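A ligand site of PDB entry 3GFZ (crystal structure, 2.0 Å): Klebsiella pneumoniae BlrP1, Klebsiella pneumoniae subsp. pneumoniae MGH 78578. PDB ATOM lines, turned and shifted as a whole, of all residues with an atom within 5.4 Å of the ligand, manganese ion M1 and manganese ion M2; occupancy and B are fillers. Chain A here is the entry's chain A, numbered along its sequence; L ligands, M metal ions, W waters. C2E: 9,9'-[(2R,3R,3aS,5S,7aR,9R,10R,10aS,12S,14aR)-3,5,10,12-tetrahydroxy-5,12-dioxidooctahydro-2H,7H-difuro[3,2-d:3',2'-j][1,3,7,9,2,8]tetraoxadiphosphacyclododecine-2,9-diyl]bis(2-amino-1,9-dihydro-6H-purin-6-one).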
ATOM      1  N   PHE A 179     -12.582  18.942 -10.382  1.00  0.00           N
ATOM      2  CA  PHE A 179     -12.194  18.064  -9.290  1.00  0.00           C
ATOM      3  C   PHE A 179     -11.449  16.881  -9.840  1.00  0.00           C
ATOM      4  O   PHE A 179     -11.849  16.277 -10.844  1.00  0.00           O
ATOM      5  CB  PHE A 179     -13.409  17.592  -8.490  1.00  0.00           C
ATOM      6  CG  PHE A 179     -13.967  18.640  -7.589  1.00  0.00           C
ATOM      7  CD1 PHE A 179     -14.924  19.517  -8.048  1.00  0.00           C
ATOM      8  CD2 PHE A 179     -13.495  18.778  -6.297  1.00  0.00           C
ATOM      9  CE1 PHE A 179     -15.420  20.503  -7.235  1.00  0.00           C
ATOM     10  CE2 PHE A 179     -13.995  19.754  -5.462  1.00  0.00           C
ATOM     11  CZ  PHE A 179     -14.958  20.627  -5.928  1.00  0.00           C
ATOM     12  N   GLN A 182      -9.127  10.756  -6.368  1.00  0.00           N
ATOM     13  CA  GLN A 182      -8.140   9.764  -5.958  1.00  0.00           C
ATOM     14  C   GLN A 182      -8.857   8.659  -5.172  1.00  0.00           C
ATOM     15  O   GLN A 182      -9.647   8.940  -4.266  1.00  0.00           O
ATOM     16  CB  GLN A 182      -7.038  10.384  -5.099  1.00  0.00           C
ATOM     17  CG  GLN A 182      -5.933   9.400  -4.680  1.00  0.00           C
ATOM     18  CD  GLN A 182      -4.781  10.078  -3.943  1.00  0.00           C
ATOM     19  OE1 GLN A 182      -4.974  11.031  -3.191  1.00  0.00           O
ATOM     20  NE2 GLN A 182      -3.574   9.576  -4.161  1.00  0.00           N
ATOM     21  N   GLU A 196     -11.801  10.319  -3.122  1.00  0.00           N
ATOM     22  CA  GLU A 196     -11.735  11.679  -2.594  1.00  0.00           C
ATOM     23  C   GLU A 196     -11.716  12.691  -3.734  1.00  0.00           C
ATOM     24  O   GLU A 196     -10.923  12.563  -4.648  1.00  0.00           O
ATOM     25  CB  GLU A 196     -10.510  11.904  -1.713  1.00  0.00           C
ATOM     26  CG  GLU A 196     -10.427  13.333  -1.219  1.00  0.00           C
ATOM     27  CD  GLU A 196      -9.372  13.576  -0.169  1.00  0.00           C
ATOM     28  OE1 GLU A 196      -8.529  12.686   0.074  1.00  0.00           O
ATOM     29  OE2 GLU A 196      -9.432  14.684   0.429  1.00  0.00           O
ATOM     30  N   ALA A 197     -12.577  13.709  -3.628  1.00  0.00           N
ATOM     31  CA  ALA A 197     -12.638  14.799  -4.591  1.00  0.00           C
ATOM     32  C   ALA A 197     -11.671  15.923  -4.179  1.00  0.00           C
ATOM     33  O   ALA A 197     -11.798  16.509  -3.114  1.00  0.00           O
ATOM     34  CB  ALA A 197     -14.050  15.327  -4.671  1.00  0.00           C
ATOM     35  N   LEU A 198     -10.726  16.225  -5.064  1.00  0.00           N
ATOM     36  CA  LEU A 198      -9.692  17.234  -4.827  1.00  0.00           C
ATOM     37  C   LEU A 198      -9.869  18.380  -5.820  1.00  0.00           C
ATOM     38  O   LEU A 198      -9.767  18.171  -7.017  1.00  0.00           O
ATOM     39  CB  LEU A 198      -8.316  16.601  -4.996  1.00  0.00           C
ATOM     40  CG  LEU A 198      -8.067  15.342  -4.171  1.00  0.00           C
ATOM     41  CD1 LEU A 198      -6.776  14.649  -4.598  1.00  0.00           C
ATOM     42  CD2 LEU A 198      -8.076  15.677  -2.671  1.00  0.00           C
ATOM     43  N   ILE A 199     -10.117  19.593  -5.314  1.00  0.00           N
ATOM     44  CA  ILE A 199     -10.498  20.701  -6.193  1.00  0.00           C
ATOM     45  C   ILE A 199      -9.340  21.150  -7.059  1.00  0.00           C
ATOM     46  O   ILE A 199      -8.179  21.144  -6.632  1.00  0.00           O
ATOM     47  CB  ILE A 199     -11.064  21.906  -5.401  1.00  0.00           C
ATOM     48  CG1 ILE A 199     -11.876  22.835  -6.330  1.00  0.00           C
ATOM     49  CG2 ILE A 199      -9.944  22.677  -4.683  1.00  0.00           C
ATOM     50  CD1 ILE A 199     -12.780  23.792  -5.572  1.00  0.00           C
ATOM     51  N   ARG A 200      -9.667  21.544  -8.284  1.00  0.00           N
ATOM     52  CA  ARG A 200      -8.701  22.006  -9.262  1.00  0.00           C
ATOM     53  C   ARG A 200      -9.218  23.261  -9.926  1.00  0.00           C
ATOM     54  O   ARG A 200     -10.422  23.515  -9.932  1.00  0.00           O
ATOM     55  CB  ARG A 200      -8.484  20.924 -10.312  1.00  0.00           C
ATOM     56  CG  ARG A 200      -7.910  19.642  -9.777  1.00  0.00           C
ATOM     57  CD  ARG A 200      -6.429  19.776  -9.562  1.00  0.00           C
ATOM     58  NE  ARG A 200      -5.843  18.570  -8.990  1.00  0.00           N
ATOM     59  CZ  ARG A 200      -5.723  18.307  -7.690  1.00  0.00           C
ATOM     60  NH1 ARG A 200      -6.118  19.174  -6.777  1.00  0.00           N
ATOM     61  NH2 ARG A 200      -5.169  17.160  -7.312  1.00  0.00           N
ATOM     62  N   SER A 206      -3.624  23.629  -9.010  1.00  0.00           N
ATOM     63  CA  SER A 206      -3.784  23.148  -7.629  1.00  0.00           C
ATOM     64  C   SER A 206      -4.907  23.881  -6.876  1.00  0.00           C
ATOM     65  O   SER A 206      -5.360  24.928  -7.342  1.00  0.00           O
ATOM     66  CB  SER A 206      -2.468  23.353  -6.866  1.00  0.00           C
ATOM     67  OG  SER A 206      -2.217  24.753  -6.696  1.00  0.00           O
ATOM     68  N   PRO A 207      -5.346  23.339  -5.721  1.00  0.00           N
ATOM     69  CA  PRO A 207      -6.331  24.024  -4.865  1.00  0.00           C
ATOM     70  C   PRO A 207      -5.903  25.434  -4.459  1.00  0.00           C
ATOM     71  O   PRO A 207      -6.737  26.344  -4.419  1.00  0.00           O
ATOM     72  CB  PRO A 207      -6.416  23.118  -3.627  1.00  0.00           C
ATOM     73  CG  PRO A 207      -6.057  21.789  -4.127  1.00  0.00           C
ATOM     74  CD  PRO A 207      -4.973  22.034  -5.137  1.00  0.00           C
ATOM     75  N   PHE A 211      -8.095  28.684  -5.188  1.00  0.00           N
ATOM     76  CA  PHE A 211      -8.569  29.631  -4.169  1.00  0.00           C
ATOM     77  C   PHE A 211      -7.932  31.020  -4.234  1.00  0.00           C
ATOM     78  O   PHE A 211      -8.542  31.993  -3.801  1.00  0.00           O
ATOM     79  CB  PHE A 211      -8.439  29.047  -2.765  1.00  0.00           C
ATOM     80  CG  PHE A 211      -9.528  28.084  -2.419  1.00  0.00           C
ATOM     81  CD1 PHE A 211     -10.809  28.541  -2.146  1.00  0.00           C
ATOM     82  CD2 PHE A 211      -9.290  26.724  -2.370  1.00  0.00           C
ATOM     83  CE1 PHE A 211     -11.828  27.669  -1.831  1.00  0.00           C
ATOM     84  CE2 PHE A 211     -10.305  25.844  -2.054  1.00  0.00           C
ATOM     85  CZ  PHE A 211     -11.578  26.315  -1.781  1.00  0.00           C
ATOM     86  N   ASP A 223     -15.920  27.599  -1.562  1.00  0.00           N
ATOM     87  CA  ASP A 223     -15.532  26.258  -1.123  1.00  0.00           C
ATOM     88  C   ASP A 223     -16.746  25.362  -1.023  1.00  0.00           C
ATOM     89  O   ASP A 223     -16.738  24.216  -1.494  1.00  0.00           O
ATOM     90  CB  ASP A 223     -14.836  26.348   0.245  1.00  0.00           C
ATOM     91  CG  ASP A 223     -14.341  25.005   0.736  1.00  0.00           C
ATOM     92  OD1 ASP A 223     -14.030  24.146  -0.099  1.00  0.00           O
ATOM     93  OD2 ASP A 223     -14.267  24.802   1.976  1.00  0.00           O
ATOM     94  N   SER A 226     -18.694  25.040  -4.586  1.00  0.00           N
ATOM     95  CA  SER A 226     -17.945  24.212  -5.514  1.00  0.00           C
ATOM     96  C   SER A 226     -18.322  22.737  -5.437  1.00  0.00           C
ATOM     97  O   SER A 226     -18.130  22.008  -6.390  1.00  0.00           O
ATOM     98  CB  SER A 226     -16.431  24.340  -5.281  1.00  0.00           C
ATOM     99  OG  SER A 226     -16.038  23.757  -4.046  1.00  0.00           O
ATOM    100  N   LYS A 227     -18.864  22.313  -4.296  1.00  0.00           N
ATOM    101  CA  LYS A 227     -19.191  20.902  -4.072  1.00  0.00           C
ATOM    102  C   LYS A 227     -20.294  20.342  -4.973  1.00  0.00           C
ATOM    103  O   LYS A 227     -20.341  19.139  -5.208  1.00  0.00           O
ATOM    104  CB  LYS A 227     -19.491  20.662  -2.584  1.00  0.00           C
ATOM    105  CG  LYS A 227     -18.315  20.995  -1.647  1.00  0.00           C
ATOM    106  CD  LYS A 227     -16.997  20.430  -2.185  1.00  0.00           C
ATOM    107  CE  LYS A 227     -15.840  20.738  -1.289  1.00  0.00           C
ATOM    108  NZ  LYS A 227     -15.239  22.084  -1.482  1.00  0.00           N
ATOM    109  N   ASN A 247     -13.662  17.633   0.858  1.00  0.00           N
ATOM    110  CA  ASN A 247     -12.952  18.490   1.793  1.00  0.00           C
ATOM    111  C   ASN A 247     -13.677  19.813   1.946  1.00  0.00           C
ATOM    112  O   ASN A 247     -14.029  20.436   0.946  1.00  0.00           O
ATOM    113  CB  ASN A 247     -11.544  18.802   1.299  1.00  0.00           C
ATOM    114  CG  ASN A 247     -10.682  17.580   1.220  1.00  0.00           C
ATOM    115  OD1 ASN A 247     -10.197  17.094   2.240  1.00  0.00           O
ATOM    116  ND2 ASN A 247     -10.454  17.083   0.006  1.00  0.00           N
ATOM    117  N   LEU A 248     -13.883  20.258   3.182  1.00  0.00           N
ATOM    118  CA  LEU A 248     -14.517  21.557   3.438  1.00  0.00           C
ATOM    119  C   LEU A 248     -13.881  22.234   4.642  1.00  0.00           C
ATOM    120  O   LEU A 248     -13.523  21.565   5.604  1.00  0.00           O
ATOM    121  CB  LEU A 248     -16.022  21.370   3.704  1.00  0.00           C
ATOM    122  CG  LEU A 248     -16.996  21.330   2.521  1.00  0.00           C
ATOM    123  CD1 LEU A 248     -18.421  21.022   3.014  1.00  0.00           C
ATOM    124  CD2 LEU A 248     -17.004  22.632   1.742  1.00  0.00           C
ATOM    125  N   LEU A 249     -13.738  23.555   4.567  1.00  0.00           N
ATOM    126  CA  LEU A 249     -13.338  24.355   5.722  1.00  0.00           C
ATOM    127  C   LEU A 249     -14.525  24.409   6.672  1.00  0.00           C
ATOM    128  O   LEU A 249     -15.657  24.634   6.240  1.00  0.00           O
ATOM    129  CB  LEU A 249     -12.979  25.786   5.300  1.00  0.00           C
ATOM    130  CG  LEU A 249     -11.840  25.990   4.306  1.00  0.00           C
ATOM    131  CD1 LEU A 249     -11.844  27.417   3.779  1.00  0.00           C
ATOM    132  CD2 LEU A 249     -10.501  25.659   4.924  1.00  0.00           C
ATOM    133  N   GLU A 280     -14.658  15.723   4.859  1.00  0.00           N
ATOM    134  CA  GLU A 280     -13.333  15.781   5.480  1.00  0.00           C
ATOM    135  C   GLU A 280     -13.053  17.179   6.024  1.00  0.00           C
ATOM    136  O   GLU A 280     -13.064  18.144   5.271  1.00  0.00           O
ATOM    137  CB  GLU A 280     -12.226  15.415   4.497  1.00  0.00           C
ATOM    138  CG  GLU A 280     -12.378  14.030   3.900  1.00  0.00           C
ATOM    139  CD  GLU A 280     -11.095  13.465   3.309  1.00  0.00           C
ATOM    140  OE1 GLU A 280     -11.113  12.284   2.904  1.00  0.00           O
ATOM    141  OE2 GLU A 280     -10.078  14.191   3.216  1.00  0.00           O
ATOM    142  N   THR A 282     -10.051  19.072   8.514  1.00  0.00           N
ATOM    143  CA  THR A 282      -8.736  18.855   9.083  1.00  0.00           C
ATOM    144  C   THR A 282      -8.775  19.153  10.570  1.00  0.00           C
ATOM    145  O   THR A 282      -9.427  20.097  11.009  1.00  0.00           O
ATOM    146  CB  THR A 282      -7.640  19.726   8.448  1.00  0.00           C
ATOM    147  OG1 THR A 282      -8.047  21.092   8.489  1.00  0.00           O
ATOM    148  CG2 THR A 282      -7.391  19.308   7.028  1.00  0.00           C
ATOM    149  N   ASP A 310      -9.303  14.669   8.747  1.00  0.00           N
ATOM    150  CA  ASP A 310      -8.242  14.589   7.760  1.00  0.00           C
ATOM    151  C   ASP A 310      -6.945  15.026   8.441  1.00  0.00           C
ATOM    152  O   ASP A 310      -6.981  15.789   9.404  1.00  0.00           O
ATOM    153  CB  ASP A 310      -8.595  15.553   6.626  1.00  0.00           C
ATOM    154  CG  ASP A 310      -7.904  15.240   5.322  1.00  0.00           C
ATOM    155  OD1 ASP A 310      -7.159  14.226   5.198  1.00  0.00           O
ATOM    156  OD2 ASP A 310      -8.155  16.020   4.358  1.00  0.00           O
ATOM    157  N   ASP A 311      -5.819  14.527   7.944  1.00  0.00           N
ATOM    158  CA  ASP A 311      -4.491  14.911   8.462  1.00  0.00           C
ATOM    159  C   ASP A 311      -4.391  14.744   9.965  1.00  0.00           C
ATOM    160  O   ASP A 311      -3.810  15.569  10.664  1.00  0.00           O
ATOM    161  CB  ASP A 311      -4.138  16.354   8.066  1.00  0.00           C
ATOM    162  CG  ASP A 311      -4.203  16.581   6.575  1.00  0.00           C
ATOM    163  OD1 ASP A 311      -4.008  15.607   5.819  1.00  0.00           O
ATOM    164  OD2 ASP A 311      -4.433  17.731   6.169  1.00  0.00           O
ATOM    165  N   LYS A 331      -8.133   9.975   9.069  1.00  0.00           N
ATOM    166  CA  LYS A 331      -7.121   9.802   8.029  1.00  0.00           C
ATOM    167  C   LYS A 331      -5.776  10.172   8.636  1.00  0.00           C
ATOM    168  O   LYS A 331      -5.563  11.318   8.984  1.00  0.00           O
ATOM    169  CB  LYS A 331      -7.460  10.651   6.815  1.00  0.00           C
ATOM    170  CG  LYS A 331      -8.878  10.419   6.324  1.00  0.00           C
ATOM    171  CD  LYS A 331      -9.167  11.146   5.020  1.00  0.00           C
ATOM    172  CE  LYS A 331      -8.667  10.353   3.838  1.00  0.00           C
ATOM    173  NZ  LYS A 331      -9.248  10.805   2.556  1.00  0.00           N
ATOM    174  N   GLU A 367      -2.749   8.077   4.760  1.00  0.00           N
ATOM    175  CA  GLU A 367      -2.520   8.974   3.643  1.00  0.00           C
ATOM    176  C   GLU A 367      -1.056   9.058   3.240  1.00  0.00           C
ATOM    177  O   GLU A 367      -0.180   8.865   4.066  1.00  0.00           O
ATOM    178  CB  GLU A 367      -2.893  10.408   3.995  1.00  0.00           C
ATOM    179  CG  GLU A 367      -4.260  10.661   4.487  1.00  0.00           C
ATOM    180  CD  GLU A 367      -4.549  12.150   4.499  1.00  0.00           C
ATOM    181  OE1 GLU A 367      -4.710  12.719   3.401  1.00  0.00           O
ATOM    182  OE2 GLU A 367      -4.590  12.765   5.590  1.00  0.00           O
ATOM    183  N   GLY A 368      -0.826   9.433   1.989  1.00  0.00           N
ATOM    184  CA  GLY A 368       0.525   9.732   1.505  1.00  0.00           C
ATOM    185  C   GLY A 368       1.408   8.508   1.343  1.00  0.00           C
ATOM    186  O   GLY A 368       2.622   8.612   1.457  1.00  0.00           O
ATOM    187  N   VAL A 369       0.788   7.371   1.042  1.00  0.00           N
ATOM    188  CA  VAL A 369       1.512   6.097   0.934  1.00  0.00           C
ATOM    189  C   VAL A 369       2.185   6.017  -0.452  1.00  0.00           C
ATOM    190  O   VAL A 369       1.509   5.874  -1.470  1.00  0.00           O
ATOM    191  CB  VAL A 369       0.567   4.885   1.175  1.00  0.00           C
ATOM    192  CG1 VAL A 369       1.352   3.595   1.232  1.00  0.00           C
ATOM    193  CG2 VAL A 369      -0.188   5.041   2.482  1.00  0.00           C
ATOM    194  N   GLU A 370       3.503   6.126  -0.464  1.00  0.00           N
ATOM    195  CA  GLU A 370       4.289   6.261  -1.676  1.00  0.00           C
ATOM    196  C   GLU A 370       5.119   5.041  -2.043  1.00  0.00           C
ATOM    197  O   GLU A 370       5.495   4.888  -3.199  1.00  0.00           O
ATOM    198  CB  GLU A 370       5.216   7.474  -1.533  1.00  0.00           C
ATOM    199  CG  GLU A 370       4.464   8.767  -1.358  1.00  0.00           C
ATOM    200  CD  GLU A 370       5.338   9.998  -1.401  1.00  0.00           C
ATOM    201  OE1 GLU A 370       6.568   9.908  -1.151  1.00  0.00           O
ATOM    202  OE2 GLU A 370       4.786  11.074  -1.665  1.00  0.00           O
ATOM    203  N   GLN A 387      -4.429   5.516   0.972  1.00  0.00           N
ATOM    204  CA  GLN A 387      -4.546   6.543  -0.040  1.00  0.00           C
ATOM    205  C   GLN A 387      -3.133   7.016  -0.329  1.00  0.00           C
ATOM    206  O   GLN A 387      -2.404   7.426   0.560  1.00  0.00           O
ATOM    207  CB  GLN A 387      -5.403   7.685   0.483  1.00  0.00           C
ATOM    208  CG  GLN A 387      -5.809   8.677  -0.608  1.00  0.00           C
ATOM    209  CD  GLN A 387      -6.642   9.797  -0.082  1.00  0.00           C
ATOM    210  OE1 GLN A 387      -7.130   9.746   1.056  1.00  0.00           O
ATOM    211  NE2 GLN A 387      -6.827  10.834  -0.893  1.00  0.00           N
ATOM    212  N   GLY A 388      -2.736   6.934  -1.590  1.00  0.00           N
ATOM    213  CA  GLY A 388      -1.441   7.423  -1.956  1.00  0.00           C
ATOM    214  C   GLY A 388      -1.100   7.098  -3.384  1.00  0.00           C
ATOM    215  O   GLY A 388      -1.739   6.256  -4.029  1.00  0.00           O
ATOM    216  N   PHE A 389      -0.054   7.762  -3.854  1.00  0.00           N
ATOM    217  CA  PHE A 389       0.437   7.599  -5.205  1.00  0.00           C
ATOM    218  C   PHE A 389       0.903   6.177  -5.515  1.00  0.00           C
ATOM    219  O   PHE A 389       0.977   5.797  -6.676  1.00  0.00           O
ATOM    220  CB  PHE A 389       1.591   8.559  -5.452  1.00  0.00           C
ATOM    221  CG  PHE A 389       1.217  10.028  -5.403  1.00  0.00           C
ATOM    222  CD1 PHE A 389      -0.098  10.461  -5.516  1.00  0.00           C
ATOM    223  CD2 PHE A 389       2.213  10.973  -5.271  1.00  0.00           C
ATOM    224  CE1 PHE A 389      -0.398  11.815  -5.499  1.00  0.00           C
ATOM    225  CE2 PHE A 389       1.906  12.325  -5.247  1.00  0.00           C
ATOM    226  CZ  PHE A 389       0.610  12.733  -5.363  1.00  0.00           C
ATOM    227  N   LEU A 390       1.234   5.386  -4.486  1.00  0.00           N
ATOM    228  CA  LEU A 390       1.576   3.991  -4.695  1.00  0.00           C
ATOM    229  C   LEU A 390       0.455   3.221  -5.398  1.00  0.00           C
ATOM    230  O   LEU A 390       0.713   2.399  -6.278  1.00  0.00           O
ATOM    231  CB  LEU A 390       1.914   3.310  -3.369  1.00  0.00           C
ATOM    232  CG  LEU A 390       2.435   1.864  -3.464  1.00  0.00           C
ATOM    233  CD1 LEU A 390       3.825   1.835  -4.069  1.00  0.00           C
ATOM    234  CD2 LEU A 390       2.432   1.218  -2.102  1.00  0.00           C
ATOM    235  N   PRO A 394      -4.331  11.080  -8.317  1.00  0.00           N
ATOM    236  CA  PRO A 394      -5.536  11.837  -8.645  1.00  0.00           C
ATOM    237  C   PRO A 394      -5.712  12.003 -10.154  1.00  0.00           C
ATOM    238  O   PRO A 394      -4.733  12.209 -10.885  1.00  0.00           O
ATOM    239  CB  PRO A 394      -5.296  13.190  -7.993  1.00  0.00           C
ATOM    240  CG  PRO A 394      -4.357  12.909  -6.888  1.00  0.00           C
ATOM    241  CD  PRO A 394      -3.462  11.839  -7.393  1.00  0.00           C
HETATM  242  P1  C2E L   1      -5.787  16.474   1.540  1.00  0.00           P
HETATM  243  O2P C2E L   1      -7.300  16.474   1.438  1.00  0.00           O
HETATM  244  O1P C2E L   1      -5.203  16.185   2.891  1.00  0.00           O
HETATM  245  O5' C2E L   1      -5.095  15.325   0.689  1.00  0.00           O
HETATM  246  C5' C2E L   1      -4.988  15.233  -0.705  1.00  0.00           C
HETATM  247  C4' C2E L   1      -3.606  15.726  -1.156  1.00  0.00           C
HETATM  248  O4' C2E L   1      -2.505  14.831  -0.953  1.00  0.00           O
HETATM  249  C3' C2E L   1      -3.695  15.865  -2.654  1.00  0.00           C
HETATM  250  O3' C2E L   1      -2.992  17.011  -3.025  1.00  0.00           O
HETATM  251  C2' C2E L   1      -2.949  14.717  -3.193  1.00  0.00           C
HETATM  252  O2' C2E L   1      -2.730  14.750  -4.504  1.00  0.00           O
HETATM  253  C1' C2E L   1      -2.056  14.348  -2.269  1.00  0.00           C
HETATM  254  N9  C2E L   1      -1.534  13.083  -2.246  1.00  0.00           N
HETATM  255  C8  C2E L   1      -2.274  12.031  -2.274  1.00  0.00           C
HETATM  256  N7  C2E L   1      -1.490  10.994  -2.200  1.00  0.00           N
HETATM  257  C5  C2E L   1      -0.203  11.392  -2.093  1.00  0.00           C
HETATM  258  C6  C2E L   1       1.022  10.722  -1.987  1.00  0.00           C
HETATM  259  O6  C2E L   1       1.096   9.476  -1.957  1.00  0.00           O
HETATM  260  N1  C2E L   1       2.134  11.458  -1.901  1.00  0.00           N
HETATM  261  C2  C2E L   1       2.093  12.807  -1.924  1.00  0.00           C
HETATM  262  N2  C2E L   1       3.271  13.461  -1.839  1.00  0.00           N
HETATM  263  N3  C2E L   1       0.931  13.492  -2.034  1.00  0.00           N
HETATM  264  C4  C2E L   1      -0.229  12.779  -2.119  1.00  0.00           C
HETATM  265  P11 C2E L   1      -3.839  18.270  -3.441  1.00  0.00           P
HETATM  266  O21 C2E L   1      -2.857  19.167  -4.325  1.00  0.00           O
HETATM  267  O11 C2E L   1      -5.001  17.784  -4.412  1.00  0.00           O
HETATM  268  O5A C2E L   1      -4.649  18.864  -2.189  1.00  0.00           O
HETATM  269  C5A C2E L   1      -3.999  19.778  -1.300  1.00  0.00           C
HETATM  270  C4A C2E L   1      -5.049  19.943  -0.199  1.00  0.00           C
HETATM  271  O4A C2E L   1      -5.964  20.976  -0.535  1.00  0.00           O
HETATM  272  C3A C2E L   1      -5.930  18.759   0.209  1.00  0.00           C
HETATM  273  O3A C2E L   1      -5.222  17.913   1.099  1.00  0.00           O
HETATM  274  C2A C2E L   1      -7.112  19.467   0.802  1.00  0.00           C
HETATM  275  O2A C2E L   1      -6.788  20.030   1.981  1.00  0.00           O
HETATM  276  C1A C2E L   1      -7.225  20.406  -0.144  1.00  0.00           C
HETATM  277  N91 C2E L   1      -8.397  20.571  -0.816  1.00  0.00           N
HETATM  278  C81 C2E L   1      -8.606  19.838  -1.911  1.00  0.00           C
HETATM  279  N71 C2E L   1      -9.862  20.168  -2.322  1.00  0.00           N
HETATM  280  C51 C2E L   1     -10.383  21.083  -1.468  1.00  0.00           C
HETATM  281  C61 C2E L   1     -11.599  21.733  -1.422  1.00  0.00           C
HETATM  282  O61 C2E L   1     -12.462  21.510  -2.292  1.00  0.00           O
HETATM  283  N11 C2E L   1     -11.836  22.615  -0.411  1.00  0.00           N
HETATM  284  C21 C2E L   1     -10.892  22.841   0.544  1.00  0.00           C
HETATM  285  N21 C2E L   1     -11.125  23.714   1.557  1.00  0.00           N
HETATM  286  N31 C2E L   1      -9.700  22.206   0.523  1.00  0.00           N
HETATM  287  C41 C2E L   1      -9.434  21.328  -0.472  1.00  0.00           C
HETATM  288 MN    MN M   1      -8.785  15.390   2.444  1.00  0.00          MN
HETATM  289 MN    MN M   2      -5.041  14.696   4.224  1.00  0.00          MN
HETATM  290  O   HOH W   1      -2.897  10.592   0.495  1.00  0.00           O
HETATM  291  O   HOH W   2      -7.325  13.593   2.627  1.00  0.00           O
HETATM  292  O   HOH W   3     -13.075  18.500  -1.979  1.00  0.00           O
HETATM  293  O   HOH W   4      -1.001  16.440  -5.284  1.00  0.00           O
HETATM  294  O   HOH W   5      -6.730  18.379   4.048  1.00  0.00           O
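The backbone carbonyl oxygen of Asn 247 is in hydrogen-bond range of a nitrogen (N11) of the ligand, at 3.4 Å.
OE2 of Glu 370 sits at hydrogen-bond distance from N1 of the ligand.
N11 of the ligand sits at hydrogen-bond distance from OD1 of Asp 223 (2.7 Å).
An oxygen (O6) of the ligand sits at hydrogen-bond distance from the backbone NH (N) of Phe 389, at 2.8 Å.
NZ of Lys 227 sits at hydrogen-bond distance from O61 of the ligand (2.9 Å).
The guanidinium group (NH1) of Arg 200 lies within salt-bridge range of an oxygen (O11) of the ligand (3.0 Å).
The side-chain amide nitrogen (NE2) of Gln 182 is in hydrogen-bond range of a nitrogen (N7) of the ligand (3.2 Å).
N71 of the ligand sits at hydrogen-bond distance from N of Ile 199, 3.1 Å away.
The side-chain amino group (NZ) of Lys 227 lies close to the backbone carbonyl oxygen (O) of Asn 247, 3.2 Å away.
O of Gln 182 sits at hydrogen-bond distance from N of Glu 196, 2.8 Å away.
OE1 of Glu 196 lies within hydrogen-bond range of NE2 of Gln 387 (2.7 Å).
OD1 of Asp 223 lies within salt-bridge range of NZ of Lys 227 (2.8 Å).
The side-chain carboxylate (OD2) of Asp 223 is in hydrogen-bond range of the backbone NH (N) of Leu 249 (2.9 Å).
The backbone carbonyl oxygen (O) of Asp 223 is in hydrogen-bond range of the side-chain hydroxyl (OG) of Ser 226.
NZ of Lys 227 is in hydrogen-bond range of OG of Ser 226 (3.2 Å).
O of Val 369 sits at hydrogen-bond distance from N of Leu 390.
Residues that only touch the ligand: Phe 179 (3.9 Å), Leu 198 (3.6 Å), Pro 207 (3.7 Å), Phe 211 (3.9 Å), Leu 249 (3.6 Å), Gly 368 (3.5 Å), Val 369 (3.7 Å), Gly 388 (3.3 Å) and Pro 394 (3.4 Å).
Hydrophobic or aromatic side chains within 4 Å of the ligand: Phe 179, Leu 198, Ile 199, Pro 207, Phe 211, Leu 249, Phe 389 and Pro 394.
Within 4 Å of manganese ion M1: Glu 196, Asn 247, Glu 280 and Asp 310.
The nearest printed residue that does not touch manganese ion M1 is Lys 331 (4.6 Å).
Of the 30 residues printed, 3 come within 4 Å of manganese ion M2.
Along chain A the residues within 4 Å of manganese ion M2 span positions 310 to 367.
The nearest printed residue that does not touch manganese ion M2 is Glu 280 (5.2 Å).
OE2 of Glu 280 is bound to manganese ion M1 (1.9 Å).
O2P of the ligand is bound to manganese ion M1 (2.1 Å).
Manganese ion M1 is bound by OD2 of Asp 310.
Manganese ion M1 is bound by the side-chain amide oxygen (OD1) of Asn 247.
Manganese ion M1 is bound by OE2 of Glu 196, at 2.2 Å.
Water W2 is bound to manganese ion M1 (2.3 Å).
Manganese ion M2 is bound by an oxygen (O1P) of the ligand (2.0 Å).
OD1 of Asp 311 is bound to manganese ion M2 (2.1 Å).
OE1 of Glu 367 binds manganese ion M2, at 2.2 Å.
OD1 of Asp 310 binds manganese ion M2.
The side-chain carboxylate (OE2) of Glu 367 is bound to manganese ion M2, at 2.4 Å.
Manganese ion M2 has five donor atoms within binding distance.
Water W2 lies within hydrogen-bond range of the side-chain carboxylate of Glu 196, the side-chain amino group of Lys 331 and an oxygen (O5') of the ligand.
Water W5 lies within hydrogen-bond range of O2A of the ligand and OD2 of Asp 311.
Water W1 lies within hydrogen-bond range of N of Gly 368, N7 of the ligand and O of Gln 387.
Water W3 lies within hydrogen-bond range of O of Ala 197 (2.6 Å), N of Asn 247 (3.0 Å) and O61 of the ligand (3.1 Å).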
